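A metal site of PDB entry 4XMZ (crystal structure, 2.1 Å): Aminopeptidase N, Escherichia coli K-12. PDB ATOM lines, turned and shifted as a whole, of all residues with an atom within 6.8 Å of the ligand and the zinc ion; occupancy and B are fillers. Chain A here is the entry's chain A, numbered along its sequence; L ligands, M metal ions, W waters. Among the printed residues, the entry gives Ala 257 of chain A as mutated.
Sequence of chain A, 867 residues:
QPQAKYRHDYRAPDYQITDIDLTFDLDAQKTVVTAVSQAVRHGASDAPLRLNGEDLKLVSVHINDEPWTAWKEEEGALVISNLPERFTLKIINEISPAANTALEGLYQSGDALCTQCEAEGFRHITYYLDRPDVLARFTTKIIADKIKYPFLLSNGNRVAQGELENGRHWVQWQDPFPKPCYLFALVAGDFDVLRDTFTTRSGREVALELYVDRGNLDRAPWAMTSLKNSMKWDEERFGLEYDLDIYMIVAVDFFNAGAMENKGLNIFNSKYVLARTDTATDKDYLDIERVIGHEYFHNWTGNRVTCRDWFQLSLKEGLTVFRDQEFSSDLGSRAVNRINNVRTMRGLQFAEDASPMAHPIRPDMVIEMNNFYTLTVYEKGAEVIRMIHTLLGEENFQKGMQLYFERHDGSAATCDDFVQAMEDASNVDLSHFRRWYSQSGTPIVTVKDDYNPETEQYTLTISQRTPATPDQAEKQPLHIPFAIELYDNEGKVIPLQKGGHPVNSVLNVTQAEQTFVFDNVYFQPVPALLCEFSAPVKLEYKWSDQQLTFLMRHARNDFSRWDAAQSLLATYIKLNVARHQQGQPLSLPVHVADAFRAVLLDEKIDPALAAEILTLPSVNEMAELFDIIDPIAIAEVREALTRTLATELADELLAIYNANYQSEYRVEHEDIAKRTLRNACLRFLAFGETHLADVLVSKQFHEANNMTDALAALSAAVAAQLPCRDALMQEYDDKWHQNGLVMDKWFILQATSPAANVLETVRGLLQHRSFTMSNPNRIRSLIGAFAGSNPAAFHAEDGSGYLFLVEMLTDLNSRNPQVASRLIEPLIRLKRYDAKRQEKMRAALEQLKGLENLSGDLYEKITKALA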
ATOM      1  N   GLN A 116      -3.481   5.427  21.177  1.00  0.00           N
ATOM      2  CA  GLN A 116      -2.291   5.065  21.945  1.00  0.00           C
ATOM      3  C   GLN A 116      -1.696   3.743  21.421  1.00  0.00           C
ATOM      4  O   GLN A 116      -2.356   2.706  21.519  1.00  0.00           O
ATOM      5  CB  GLN A 116      -2.591   4.982  23.443  1.00  0.00           C
ATOM      6  CG  GLN A 116      -1.431   4.460  24.306  1.00  0.00           C
ATOM      7  CD  GLN A 116      -0.218   5.360  24.233  1.00  0.00           C
ATOM      8  OE1 GLN A 116      -0.356   6.586  24.098  1.00  0.00           O
ATOM      9  NE2 GLN A 116       0.967   4.766  24.323  1.00  0.00           N
ATOM     10  N   GLU A 118       1.908   2.724  21.830  1.00  0.00           N
ATOM     11  CA  GLU A 118       2.978   2.079  22.592  1.00  0.00           C
ATOM     12  C   GLU A 118       2.378   1.226  23.700  1.00  0.00           C
ATOM     13  O   GLU A 118       1.483   1.694  24.406  1.00  0.00           O
ATOM     14  CB  GLU A 118       3.971   3.068  23.217  1.00  0.00           C
ATOM     15  CG  GLU A 118       5.129   2.357  23.874  1.00  0.00           C
ATOM     16  CD  GLU A 118       6.217   3.265  24.431  1.00  0.00           C
ATOM     17  OE1 GLU A 118       6.015   4.475  24.425  1.00  0.00           O
ATOM     18  OE2 GLU A 118       7.287   2.769  24.843  1.00  0.00           O
ATOM     19  N   TYR A 182       4.772   2.266  16.885  1.00  0.00           N
ATOM     20  CA  TYR A 182       4.342   2.698  18.212  1.00  0.00           C
ATOM     21  C   TYR A 182       4.321   4.204  18.362  1.00  0.00           C
ATOM     22  O   TYR A 182       3.762   4.763  19.328  1.00  0.00           O
ATOM     23  CB  TYR A 182       5.178   2.087  19.314  1.00  0.00           C
ATOM     24  CG  TYR A 182       6.510   2.704  19.613  1.00  0.00           C
ATOM     25  CD1 TYR A 182       6.599   3.808  20.465  1.00  0.00           C
ATOM     26  CD2 TYR A 182       7.705   2.183  19.052  1.00  0.00           C
ATOM     27  CE1 TYR A 182       7.850   4.366  20.808  1.00  0.00           C
ATOM     28  CE2 TYR A 182       8.962   2.758  19.327  1.00  0.00           C
ATOM     29  CZ  TYR A 182       9.029   3.832  20.220  1.00  0.00           C
ATOM     30  OH  TYR A 182      10.225   4.424  20.486  1.00  0.00           O
ATOM     31  N   PHE A 255      -6.818   8.571  29.380  1.00  0.00           N
ATOM     32  CA  PHE A 255      -5.476   8.163  28.963  1.00  0.00           C
ATOM     33  C   PHE A 255      -4.885   7.302  30.074  1.00  0.00           C
ATOM     34  O   PHE A 255      -4.952   7.666  31.274  1.00  0.00           O
ATOM     35  CB  PHE A 255      -4.621   9.439  28.675  1.00  0.00           C
ATOM     36  CG  PHE A 255      -3.448   9.210  27.776  1.00  0.00           C
ATOM     37  CD1 PHE A 255      -3.609   9.003  26.435  1.00  0.00           C
ATOM     38  CD2 PHE A 255      -2.144   9.188  28.291  1.00  0.00           C
ATOM     39  CE1 PHE A 255      -2.538   8.869  25.565  1.00  0.00           C
ATOM     40  CE2 PHE A 255      -1.049   9.002  27.423  1.00  0.00           C
ATOM     41  CZ  PHE A 255      -1.261   8.840  26.063  1.00  0.00           C
ATOM     42  N   ASN A 256      -4.332   6.158  29.715  1.00  0.00           N
ATOM     43  CA  ASN A 256      -3.742   5.250  30.698  1.00  0.00           C
ATOM     44  C   ASN A 256      -2.375   5.673  31.256  1.00  0.00           C
ATOM     45  O   ASN A 256      -2.117   5.485  32.447  1.00  0.00           O
ATOM     46  CB  ASN A 256      -3.618   3.822  30.133  1.00  0.00           C
ATOM     47  CG  ASN A 256      -4.948   3.063  30.167  1.00  0.00           C
ATOM     48  OD1 ASN A 256      -5.843   3.344  30.992  1.00  0.00           O
ATOM     49  ND2 ASN A 256      -5.112   2.119  29.243  1.00  0.00           N
ATOM     50  N   ALA A 257      -1.507   6.175  30.409  1.00  0.00           N
ATOM     51  CA  ALA A 257      -0.214   6.703  30.842  1.00  0.00           C
ATOM     52  C   ALA A 257      -0.326   8.186  31.353  1.00  0.00           C
ATOM     53  O   ALA A 257      -1.452   8.733  31.650  1.00  0.00           O
ATOM     54  CB  ALA A 257       0.767   6.622  29.671  1.00  0.00           C
ATOM     55  N   GLY A 258       0.822   8.810  31.498  1.00  0.00           N
ATOM     56  CA  GLY A 258       0.933  10.208  31.714  1.00  0.00           C
ATOM     57  C   GLY A 258       0.897  10.908  30.360  1.00  0.00           C
ATOM     58  O   GLY A 258       0.148  11.883  30.179  1.00  0.00           O
ATOM     59  N   ALA A 259       1.717  10.426  29.447  1.00  0.00           N
ATOM     60  CA  ALA A 259       1.825  11.088  28.177  1.00  0.00           C
ATOM     61  C   ALA A 259       2.649  10.270  27.183  1.00  0.00           C
ATOM     62  O   ALA A 259       3.247   9.267  27.555  1.00  0.00           O
ATOM     63  CB  ALA A 259       2.465  12.462  28.374  1.00  0.00           C
ATOM     64  N   MET A 260       2.663  10.690  25.925  1.00  0.00           N
ATOM     65  CA  MET A 260       3.239   9.879  24.891  1.00  0.00           C
ATOM     66  C   MET A 260       3.915  10.723  23.830  1.00  0.00           C
ATOM     67  O   MET A 260       3.312  11.678  23.276  1.00  0.00           O
ATOM     68  CB  MET A 260       2.166   9.049  24.248  1.00  0.00           C
ATOM     69  CG  MET A 260       2.667   8.137  23.146  1.00  0.00           C
ATOM     70  SD  MET A 260       3.792   6.882  23.829  1.00  0.00           S
ATOM     71  CE  MET A 260       4.818   6.648  22.374  1.00  0.00           C
ATOM     72  N   GLU A 261       5.101  10.296  23.468  1.00  0.00           N
ATOM     73  CA  GLU A 261       5.991  11.069  22.602  1.00  0.00           C
ATOM     74  C   GLU A 261       5.826  10.918  21.088  1.00  0.00           C
ATOM     75  O   GLU A 261       6.803  10.995  20.284  1.00  0.00           O
ATOM     76  CB  GLU A 261       7.428  10.715  22.983  1.00  0.00           C
ATOM     77  CG  GLU A 261       7.870   9.303  22.615  1.00  0.00           C
ATOM     78  CD  GLU A 261       7.700   8.269  23.709  1.00  0.00           C
ATOM     79  OE1 GLU A 261       6.869   8.460  24.644  1.00  0.00           O
ATOM     80  OE2 GLU A 261       8.385   7.234  23.611  1.00  0.00           O
ATOM     81  N   VAL A 291       6.996  16.557  32.567  1.00  0.00           N
ATOM     82  CA  VAL A 291       6.492  15.602  31.620  1.00  0.00           C
ATOM     83  C   VAL A 291       6.453  16.188  30.197  1.00  0.00           C
ATOM     84  O   VAL A 291       6.748  15.496  29.241  1.00  0.00           O
ATOM     85  CB  VAL A 291       5.118  15.066  32.064  1.00  0.00           C
ATOM     86  CG1 VAL A 291       4.484  14.139  31.008  1.00  0.00           C
ATOM     87  CG2 VAL A 291       5.280  14.337  33.395  1.00  0.00           C
ATOM     88  N   HIS A 294      10.012  15.702  29.260  1.00  0.00           N
ATOM     89  CA  HIS A 294      10.247  14.301  29.019  1.00  0.00           C
ATOM     90  C   HIS A 294       9.795  13.898  27.617  1.00  0.00           C
ATOM     91  O   HIS A 294      10.598  13.351  26.893  1.00  0.00           O
ATOM     92  CB  HIS A 294       9.513  13.488  30.120  1.00  0.00           C
ATOM     93  CG  HIS A 294       9.670  12.011  29.993  1.00  0.00           C
ATOM     94  ND1 HIS A 294      10.589  11.282  30.731  1.00  0.00           N
ATOM     95  CD2 HIS A 294       9.066  11.124  29.173  1.00  0.00           C
ATOM     96  CE1 HIS A 294      10.512  10.022  30.390  1.00  0.00           C
ATOM     97  NE2 HIS A 294       9.623   9.914  29.426  1.00  0.00           N
ATOM     98  N   GLU A 295       8.547  14.195  27.218  1.00  0.00           N
ATOM     99  CA  GLU A 295       8.062  13.800  25.925  1.00  0.00           C
ATOM    100  C   GLU A 295       8.847  14.569  24.842  1.00  0.00           C
ATOM    101  O   GLU A 295       9.185  13.996  23.873  1.00  0.00           O
ATOM    102  CB  GLU A 295       6.569  14.013  25.773  1.00  0.00           C
ATOM    103  CG  GLU A 295       5.689  13.398  26.877  1.00  0.00           C
ATOM    104  CD  GLU A 295       6.029  11.928  27.256  1.00  0.00           C
ATOM    105  OE1 GLU A 295       6.646  11.222  26.408  1.00  0.00           O
ATOM    106  OE2 GLU A 295       5.751  11.520  28.430  1.00  0.00           O
ATOM    107  N   HIS A 298      12.278  12.895  24.302  1.00  0.00           N
ATOM    108  CA  HIS A 298      12.141  11.681  23.498  1.00  0.00           C
ATOM    109  C   HIS A 298      12.331  11.896  21.990  1.00  0.00           C
ATOM    110  O   HIS A 298      12.568  10.929  21.275  1.00  0.00           O
ATOM    111  CB  HIS A 298      10.774  11.012  23.705  1.00  0.00           C
ATOM    112  CG  HIS A 298      10.723   9.994  24.795  1.00  0.00           C
ATOM    113  ND1 HIS A 298      11.596   8.922  24.849  1.00  0.00           N
ATOM    114  CD2 HIS A 298       9.847   9.853  25.819  1.00  0.00           C
ATOM    115  CE1 HIS A 298      11.276   8.190  25.900  1.00  0.00           C
ATOM    116  NE2 HIS A 298      10.235   8.734  26.505  1.00  0.00           N
ATOM    117  N   THR A 301      15.952  10.976  22.094  1.00  0.00           N
ATOM    118  CA  THR A 301      16.223   9.737  22.830  1.00  0.00           C
ATOM    119  C   THR A 301      14.946   8.898  22.890  1.00  0.00           C
ATOM    120  O   THR A 301      14.213   8.904  23.889  1.00  0.00           O
ATOM    121  CB  THR A 301      16.766  10.013  24.221  1.00  0.00           C
ATOM    122  OG1 THR A 301      15.968  10.967  24.904  1.00  0.00           O
ATOM    123  CG2 THR A 301      18.154  10.616  24.053  1.00  0.00           C
ATOM    124  N   LEU A 313      13.643  -1.263  26.288  1.00  0.00           N
ATOM    125  CA  LEU A 313      12.901  -0.054  26.668  1.00  0.00           C
ATOM    126  C   LEU A 313      13.712   0.999  27.432  1.00  0.00           C
ATOM    127  O   LEU A 313      13.573   2.193  27.155  1.00  0.00           O
ATOM    128  CB  LEU A 313      11.633  -0.428  27.478  1.00  0.00           C
ATOM    129  CG  LEU A 313      10.723   0.653  27.911  1.00  0.00           C
ATOM    130  CD1 LEU A 313      10.115   1.373  26.688  1.00  0.00           C
ATOM    131  CD2 LEU A 313       9.661   0.052  28.756  1.00  0.00           C
ATOM    132  N   LYS A 316      15.552   4.084  25.924  1.00  0.00           N
ATOM    133  CA  LYS A 316      14.911   5.363  25.746  1.00  0.00           C
ATOM    134  C   LYS A 316      14.372   5.931  27.053  1.00  0.00           C
ATOM    135  O   LYS A 316      14.475   7.137  27.288  1.00  0.00           O
ATOM    136  CB  LYS A 316      13.842   5.350  24.621  1.00  0.00           C
ATOM    137  CG  LYS A 316      12.544   4.597  24.898  1.00  0.00           C
ATOM    138  CD  LYS A 316      11.636   4.696  23.702  1.00  0.00           C
ATOM    139  CE  LYS A 316      10.302   3.990  23.822  1.00  0.00           C
ATOM    140  NZ  LYS A 316       9.305   4.602  24.707  1.00  0.00           N
ATOM    141  N   GLU A 317      13.889   5.070  27.940  1.00  0.00           N
ATOM    142  CA  GLU A 317      13.263   5.597  29.158  1.00  0.00           C
ATOM    143  C   GLU A 317      14.244   5.968  30.280  1.00  0.00           C
ATOM    144  O   GLU A 317      14.074   7.018  30.969  1.00  0.00           O
ATOM    145  CB  GLU A 317      12.197   4.635  29.653  1.00  0.00           C
ATOM    146  CG  GLU A 317      11.071   4.336  28.689  1.00  0.00           C
ATOM    147  CD  GLU A 317      10.353   5.600  28.303  1.00  0.00           C
ATOM    148  OE1 GLU A 317      10.458   6.600  29.093  1.00  0.00           O
ATOM    149  OE2 GLU A 317       9.658   5.588  27.265  1.00  0.00           O
ATOM    150  N   THR A 320      15.792   9.159  28.962  1.00  0.00           N
ATOM    151  CA  THR A 320      14.882  10.308  28.838  1.00  0.00           C
ATOM    152  C   THR A 320      14.462  10.757  30.237  1.00  0.00           C
ATOM    153  O   THR A 320      14.333  11.941  30.487  1.00  0.00           O
ATOM    154  CB  THR A 320      13.712   9.974  27.921  1.00  0.00           C
ATOM    155  OG1 THR A 320      14.242   9.624  26.636  1.00  0.00           O
ATOM    156  CG2 THR A 320      12.759  11.122  27.815  1.00  0.00           C
ATOM    157  N   VAL A 321      14.312   9.819  31.177  1.00  0.00           N
ATOM    158  CA  VAL A 321      14.092  10.202  32.556  1.00  0.00           C
ATOM    159  C   VAL A 321      15.304  10.960  33.096  1.00  0.00           C
ATOM    160  O   VAL A 321      15.125  11.982  33.795  1.00  0.00           O
ATOM    161  CB  VAL A 321      13.831   9.018  33.484  1.00  0.00           C
ATOM    162  CG1 VAL A 321      13.849   9.421  34.968  1.00  0.00           C
ATOM    163  CG2 VAL A 321      12.459   8.453  33.149  1.00  0.00           C
ATOM    164  N   ASP A 324      14.977  14.451  31.727  1.00  0.00           N
ATOM    165  CA  ASP A 324      13.951  15.215  32.411  1.00  0.00           C
ATOM    166  C   ASP A 324      14.389  15.624  33.846  1.00  0.00           C
ATOM    167  O   ASP A 324      14.102  16.725  34.286  1.00  0.00           O
ATOM    168  CB  ASP A 324      12.554  14.549  32.270  1.00  0.00           C
ATOM    169  CG  ASP A 324      12.148  13.507  33.395  1.00  0.00           C
ATOM    170  OD1 ASP A 324      12.348  13.791  34.608  1.00  0.00           O
ATOM    171  OD2 ASP A 324      11.544  12.411  33.053  1.00  0.00           O
ATOM    172  N   TYR A 373       6.645  -0.948  32.051  1.00  0.00           N
ATOM    173  CA  TYR A 373       6.807   0.478  32.077  1.00  0.00           C
ATOM    174  C   TYR A 373       7.001   0.813  33.570  1.00  0.00           C
ATOM    175  O   TYR A 373       6.136   1.415  34.192  1.00  0.00           O
ATOM    176  CB  TYR A 373       5.574   1.206  31.355  1.00  0.00           C
ATOM    177  CG  TYR A 373       5.767   1.019  29.825  1.00  0.00           C
ATOM    178  CD1 TYR A 373       5.560  -0.224  29.209  1.00  0.00           C
ATOM    179  CD2 TYR A 373       6.295   2.046  29.052  1.00  0.00           C
ATOM    180  CE1 TYR A 373       5.843  -0.404  27.853  1.00  0.00           C
ATOM    181  CE2 TYR A 373       6.604   1.909  27.704  1.00  0.00           C
ATOM    182  CZ  TYR A 373       6.363   0.675  27.110  1.00  0.00           C
ATOM    183  OH  TYR A 373       6.671   0.475  25.813  1.00  0.00           O
ATOM    184  N   TYR A 378      12.392   2.848  34.325  1.00  0.00           N
ATOM    185  CA  TYR A 378      12.386   4.304  34.305  1.00  0.00           C
ATOM    186  C   TYR A 378      13.386   4.903  35.292  1.00  0.00           C
ATOM    187  O   TYR A 378      14.401   5.468  34.883  1.00  0.00           O
ATOM    188  CB  TYR A 378      10.986   4.873  34.597  1.00  0.00           C
ATOM    189  CG  TYR A 378      10.071   4.897  33.425  1.00  0.00           C
ATOM    190  CD1 TYR A 378       9.693   3.706  32.761  1.00  0.00           C
ATOM    191  CD2 TYR A 378       9.619   6.119  32.872  1.00  0.00           C
ATOM    192  CE1 TYR A 378       8.840   3.758  31.648  1.00  0.00           C
ATOM    193  CE2 TYR A 378       8.799   6.174  31.731  1.00  0.00           C
ATOM    194  CZ  TYR A 378       8.391   4.993  31.144  1.00  0.00           C
ATOM    195  OH  TYR A 378       7.617   4.993  29.996  1.00  0.00           O
ATOM    196  N   ARG A 822      -1.892  -1.991  37.274  1.00  0.00           N
ATOM    197  CA  ARG A 822      -1.307  -1.007  38.197  1.00  0.00           C
ATOM    198  C   ARG A 822      -1.859  -1.197  39.587  1.00  0.00           C
ATOM    199  O   ARG A 822      -1.109  -1.129  40.555  1.00  0.00           O
ATOM    200  CB  ARG A 822      -1.673   0.461  37.870  1.00  0.00           C
ATOM    201  CG  ARG A 822      -0.857   1.137  36.839  1.00  0.00           C
ATOM    202  CD  ARG A 822      -1.215   2.658  36.848  1.00  0.00           C
ATOM    203  NE  ARG A 822       0.039   3.401  36.693  1.00  0.00           N
ATOM    204  CZ  ARG A 822       0.531   3.866  35.549  1.00  0.00           C
ATOM    205  NH1 ARG A 822      -0.167   3.786  34.408  1.00  0.00           N
ATOM    206  NH2 ARG A 822       1.705   4.479  35.562  1.00  0.00           N
HETATM  207  N1  LIG L   1       6.669   6.242  26.242  1.00  0.00           N
HETATM  208  C1  LIG L   1       5.826   7.053  27.221  1.00  0.00           C
HETATM  209  C2  LIG L   1       6.688   7.856  28.224  1.00  0.00           C
HETATM  210  O1  LIG L   1       7.799   7.545  28.423  1.00  0.00           O
HETATM  211  C3  LIG L   1       4.817   6.117  27.914  1.00  0.00           C
HETATM  212  C4  LIG L   1       4.638   6.226  29.457  1.00  0.00           C
HETATM  213  N2  LIG L   1       3.924   5.021  30.046  1.00  0.00           N
HETATM  214  O2  LIG L   1       6.293   8.898  28.945  1.00  0.00           O
HETATM  215 ZN    ZN M   1       9.447   8.164  28.349  1.00  0.00          ZN
HETATM  216  O   HOH W   1       6.127  10.504  31.827  1.00  0.00           O
HETATM  217  O   HOH W   2       4.054   8.705  31.638  1.00  0.00           O
HETATM  218  O   HOH W   3       2.925   3.845  27.085  1.00  0.00           O
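OE2 of Glu 295 sits close to O2 of the ligand, 2.7 Å away. The side-chain carboxylate of Glu 118 is in salt-bridge range of a nitrogen (N1) of the ligand, at 2.6 Å. A nitrogen (N1) of the ligand is in salt-bridge range of the side-chain carboxylate of Glu 261. N1 of the ligand lies close to NZ of Lys 316 (3.5 Å). The side-chain hydroxyl (OH) of Tyr 378 sits close to an oxygen (O1) of the ligand.
OE1 of Glu 295 lies within hydrogen-bond range of N of Glu 261 (3.4 Å). A ring nitrogen (ND1) of His 294 is in hydrogen-bond range of the side-chain carboxylate of Asp 324 (2.8 Å). O of Lys 316 is in hydrogen-bond range of OG1 of Thr 320. OE2 of Glu 118 lies within salt-bridge range of NZ of Lys 316. A ring nitrogen (ND1) of His 298 sits at hydrogen-bond distance from the side-chain hydroxyl (OG1) of Thr 320, at 3.3 Å. The side-chain carboxylate (OE2) of Glu 317 sits close to the side-chain hydroxyl (OH) of Tyr 378. The backbone carbonyl oxygen (O) of Thr 301 is in hydrogen-bond range of a ring nitrogen (ND1) of His 298. The side-chain carboxylate (OE2) of Glu 261 lies within salt-bridge range of the side-chain amino group (NZ) of Lys 316.
O2 of the ligand sits close to O of Ala 259. Merely in contact with the ligand: Ala 257 (3.6 Å), Met 260 (3.8 Å) and Tyr 373 (3.9 Å). Of the 24 residues printed, 12 come within 4 Å of the ligand. The nearest printed residue that does not touch the ligand is Gly 258 (5.0 Å).
Tyr 378 touches the zinc ion (CE2 to ZN, 3.98 Å). The nearest printed residue that does not touch the zinc ion is Thr 320 (4.5 Å).
The zinc ion is bound by an oxygen (O1) of the ligand, the side-chain carboxylate (OE1) of Glu 317, a ring nitrogen (NE2) of His 294 and a ring nitrogen (NE2) of His 298. Slightly farther from the zinc ion lies OE2 of Glu 317 (2.8 Å).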
